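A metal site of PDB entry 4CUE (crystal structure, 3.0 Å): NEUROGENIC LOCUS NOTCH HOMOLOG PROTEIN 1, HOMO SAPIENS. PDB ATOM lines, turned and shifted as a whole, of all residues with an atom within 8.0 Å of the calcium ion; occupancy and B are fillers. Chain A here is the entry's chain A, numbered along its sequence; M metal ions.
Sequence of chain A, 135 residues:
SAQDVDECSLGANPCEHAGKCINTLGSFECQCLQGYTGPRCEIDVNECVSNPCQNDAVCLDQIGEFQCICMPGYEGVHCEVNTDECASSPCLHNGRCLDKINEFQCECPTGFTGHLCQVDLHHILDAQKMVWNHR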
ATOM      1  N   ASP A   4     -35.259 -32.340   4.729  1.00  0.00           N
ATOM      2  CA  ASP A   4     -34.869 -31.138   3.989  1.00  0.00           C
ATOM      3  C   ASP A   4     -33.445 -31.290   3.356  1.00  0.00           C
ATOM      4  O   ASP A   4     -33.242 -32.222   2.576  1.00  0.00           O
ATOM      5  CB  ASP A   4     -35.065 -29.810   4.811  1.00  0.00           C
ATOM      6  CG  ASP A   4     -35.647 -28.591   4.058  1.00  0.00           C
ATOM      7  OD1 ASP A   4     -35.860 -28.683   2.820  1.00  0.00           O
ATOM      8  OD2 ASP A   4     -35.950 -27.571   4.727  1.00  0.00           O
ATOM      9  N   VAL A   5     -32.479 -30.422   3.720  1.00  0.00           N
ATOM     10  CA  VAL A   5     -31.134 -30.311   3.133  1.00  0.00           C
ATOM     11  C   VAL A   5     -30.062 -30.398   4.211  1.00  0.00           C
ATOM     12  O   VAL A   5     -30.271 -29.894   5.321  1.00  0.00           O
ATOM     13  CB  VAL A   5     -31.028 -28.857   2.525  1.00  0.00           C
ATOM     14  CG1 VAL A   5     -29.719 -28.620   1.785  1.00  0.00           C
ATOM     15  CG2 VAL A   5     -32.223 -28.462   1.698  1.00  0.00           C
ATOM     16  N   ASP A   6     -28.861 -30.893   3.850  1.00  0.00           N
ATOM     17  CA  ASP A   6     -27.718 -30.752   4.735  1.00  0.00           C
ATOM     18  C   ASP A   6     -26.931 -29.482   4.287  1.00  0.00           C
ATOM     19  O   ASP A   6     -26.093 -29.545   3.390  1.00  0.00           O
ATOM     20  CB  ASP A   6     -26.809 -31.978   4.714  1.00  0.00           C
ATOM     21  CG  ASP A   6     -25.632 -31.875   5.652  1.00  0.00           C
ATOM     22  OD1 ASP A   6     -25.414 -30.788   6.236  1.00  0.00           O
ATOM     23  OD2 ASP A   6     -24.913 -32.879   5.811  1.00  0.00           O
ATOM     24  N   GLU A   7     -27.199 -28.336   4.937  1.00  0.00           N
ATOM     25  CA  GLU A   7     -26.536 -27.081   4.611  1.00  0.00           C
ATOM     26  C   GLU A   7     -25.014 -27.130   4.816  1.00  0.00           C
ATOM     27  O   GLU A   7     -24.278 -26.327   4.240  1.00  0.00           O
ATOM     28  CB  GLU A   7     -27.134 -25.932   5.426  1.00  0.00           C
ATOM     29  CG  GLU A   7     -28.574 -25.606   5.081  1.00  0.00           C
ATOM     30  CD  GLU A   7     -29.645 -26.329   5.885  1.00  0.00           C
ATOM     31  OE1 GLU A   7     -29.351 -27.382   6.500  1.00  0.00           O
ATOM     32  OE2 GLU A   7     -30.788 -25.841   5.896  1.00  0.00           O
ATOM     33  N   CYS A   8     -24.528 -28.097   5.624  1.00  0.00           N
ATOM     34  CA  CYS A   8     -23.094 -28.263   5.902  1.00  0.00           C
ATOM     35  C   CYS A   8     -22.395 -29.062   4.817  1.00  0.00           C
ATOM     36  O   CYS A   8     -21.192 -29.228   4.903  1.00  0.00           O
ATOM     37  CB  CYS A   8     -22.867 -28.867   7.283  1.00  0.00           C
ATOM     38  SG  CYS A   8     -23.833 -28.079   8.591  1.00  0.00           S
ATOM     39  N   ILE A  22     -23.083 -27.631  11.979  1.00  0.00           N
ATOM     40  CA  ILE A  22     -23.802 -28.807  12.474  1.00  0.00           C
ATOM     41  C   ILE A  22     -25.182 -28.866  11.828  1.00  0.00           C
ATOM     42  O   ILE A  22     -25.971 -27.929  11.971  1.00  0.00           O
ATOM     43  CB  ILE A  22     -23.842 -28.836  14.024  1.00  0.00           C
ATOM     44  CG1 ILE A  22     -22.427 -29.067  14.607  1.00  0.00           C
ATOM     45  CG2 ILE A  22     -24.816 -29.910  14.542  1.00  0.00           C
ATOM     46  CD1 ILE A  22     -22.211 -28.628  16.063  1.00  0.00           C
ATOM     47  N   ASN A  23     -25.464 -29.950  11.102  1.00  0.00           N
ATOM     48  CA  ASN A  23     -26.755 -30.047  10.433  1.00  0.00           C
ATOM     49  C   ASN A  23     -27.892 -30.381  11.378  1.00  0.00           C
ATOM     50  O   ASN A  23     -27.716 -31.159  12.302  1.00  0.00           O
ATOM     51  CB  ASN A  23     -26.713 -31.076   9.282  1.00  0.00           C
ATOM     52  CG  ASN A  23     -27.950 -31.068   8.402  1.00  0.00           C
ATOM     53  OD1 ASN A  23     -28.497 -30.013   8.065  1.00  0.00           O
ATOM     54  ND2 ASN A  23     -28.425 -32.252   8.032  1.00  0.00           N
ATOM     55  N   THR A  24     -29.052 -29.757  11.161  1.00  0.00           N
ATOM     56  CA  THR A  24     -30.294 -30.113  11.844  1.00  0.00           C
ATOM     57  C   THR A  24     -31.402 -30.359  10.803  1.00  0.00           C
ATOM     58  O   THR A  24     -31.278 -29.968   9.631  1.00  0.00           O
ATOM     59  CB  THR A  24     -30.731 -29.080  12.874  1.00  0.00           C
ATOM     60  OG1 THR A  24     -31.325 -27.940  12.254  1.00  0.00           O
ATOM     61  CG2 THR A  24     -29.640 -28.678  13.813  1.00  0.00           C
ATOM     62  N   LEU A  25     -32.494 -30.993  11.215  1.00  0.00           N
ATOM     63  CA  LEU A  25     -33.614 -31.203  10.296  1.00  0.00           C
ATOM     64  C   LEU A  25     -34.382 -29.881  10.251  1.00  0.00           C
ATOM     65  O   LEU A  25     -34.877 -29.391  11.279  1.00  0.00           O
ATOM     66  CB  LEU A  25     -34.522 -32.367  10.714  1.00  0.00           C
ATOM     67  CG  LEU A  25     -33.824 -33.681  11.102  1.00  0.00           C
ATOM     68  CD1 LEU A  25     -34.797 -34.637  11.767  1.00  0.00           C
ATOM     69  CD2 LEU A  25     -33.179 -34.373   9.895  1.00  0.00           C
ATOM     70  N   GLY A  26     -34.390 -29.271   9.068  1.00  0.00           N
ATOM     71  CA  GLY A  26     -35.069 -28.002   8.850  1.00  0.00           C
ATOM     72  C   GLY A  26     -34.169 -26.780   8.920  1.00  0.00           C
ATOM     73  O   GLY A  26     -34.566 -25.687   8.516  1.00  0.00           O
ATOM     74  N   SER A  27     -32.970 -26.936   9.453  1.00  0.00           N
ATOM     75  CA  SER A  27     -32.013 -25.834   9.539  1.00  0.00           C
ATOM     76  C   SER A  27     -30.596 -26.403   9.726  1.00  0.00           C
ATOM     77  O   SER A  27     -30.274 -27.505   9.280  1.00  0.00           O
ATOM     78  CB  SER A  27     -32.392 -24.882  10.677  1.00  0.00           C
ATOM     79  OG  SER A  27     -31.698 -23.646  10.632  1.00  0.00           O
ATOM     80  N   PHE A  28     -29.746 -25.616  10.378  1.00  0.00           N
ATOM     81  CA  PHE A  28     -28.398 -25.967  10.760  1.00  0.00           C
ATOM     82  C   PHE A  28     -27.990 -25.026  11.901  1.00  0.00           C
ATOM     83  O   PHE A  28     -28.660 -24.012  12.177  1.00  0.00           O
ATOM     84  CB  PHE A  28     -27.413 -25.872   9.572  1.00  0.00           C
ATOM     85  CG  PHE A  28     -27.170 -24.471   9.092  1.00  0.00           C
ATOM     86  CD1 PHE A  28     -28.063 -23.858   8.222  1.00  0.00           C
ATOM     87  CD2 PHE A  28     -26.058 -23.772   9.508  1.00  0.00           C
ATOM     88  CE1 PHE A  28     -27.837 -22.569   7.766  1.00  0.00           C
ATOM     89  CE2 PHE A  28     -25.863 -22.473   9.084  1.00  0.00           C
ATOM     90  CZ  PHE A  28     -26.724 -21.895   8.188  1.00  0.00           C
ATOM     91  N   GLU A  29     -26.914 -25.359  12.578  1.00  0.00           N
ATOM     92  CA  GLU A  29     -26.411 -24.527  13.662  1.00  0.00           C
ATOM     93  C   GLU A  29     -24.891 -24.423  13.563  1.00  0.00           C
ATOM     94  O   GLU A  29     -24.212 -25.300  12.988  1.00  0.00           O
ATOM     95  CB  GLU A  29     -26.872 -25.028  15.045  1.00  0.00           C
ATOM     96  CG  GLU A  29     -26.388 -26.428  15.407  1.00  0.00           C
ATOM     97  CD  GLU A  29     -27.109 -27.122  16.547  1.00  0.00           C
ATOM     98  OE1 GLU A  29     -28.153 -26.592  17.017  1.00  0.00           O
ATOM     99  OE2 GLU A  29     -26.650 -28.211  16.975  1.00  0.00           O
HETATM  100 CA    CA M   1     -30.785 -29.136   7.470  1.00  0.00          CA
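The calcium ion is bound by the backbone carbonyl oxygen of Val 5 (2.3 Å), the backbone carbonyl oxygen of Thr 24 (2.4 Å), the side-chain carboxylate of Glu 7 (2.5 Å), the backbone carbonyl oxygen of Ser 27 (2.5 Å) and the side-chain amide oxygen of Asn 23 (2.5 Å).
The calcium ion has five donor atoms within binding distance.
The side-chain hydroxyl of Thr 24 sits close to the backbone NH of Ser 27 (3.4 Å).
The backbone NH of Phe 28 is in hydrogen-bond range of the side-chain hydroxyl of Thr 24 (3.4 Å).
The backbone NH of Asn 23 lies within hydrogen-bond range of the side-chain sulfur of Cys 8.
Gly 26 touches the calcium ion.
Six residues have an atom within 4 Å of the calcium ion: Val 5, Glu 7, Asn 23, Thr 24, Gly 26 and Ser 27.
The nearest printed residue that does not touch the calcium ion is Asp 6 (4.4 Å).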
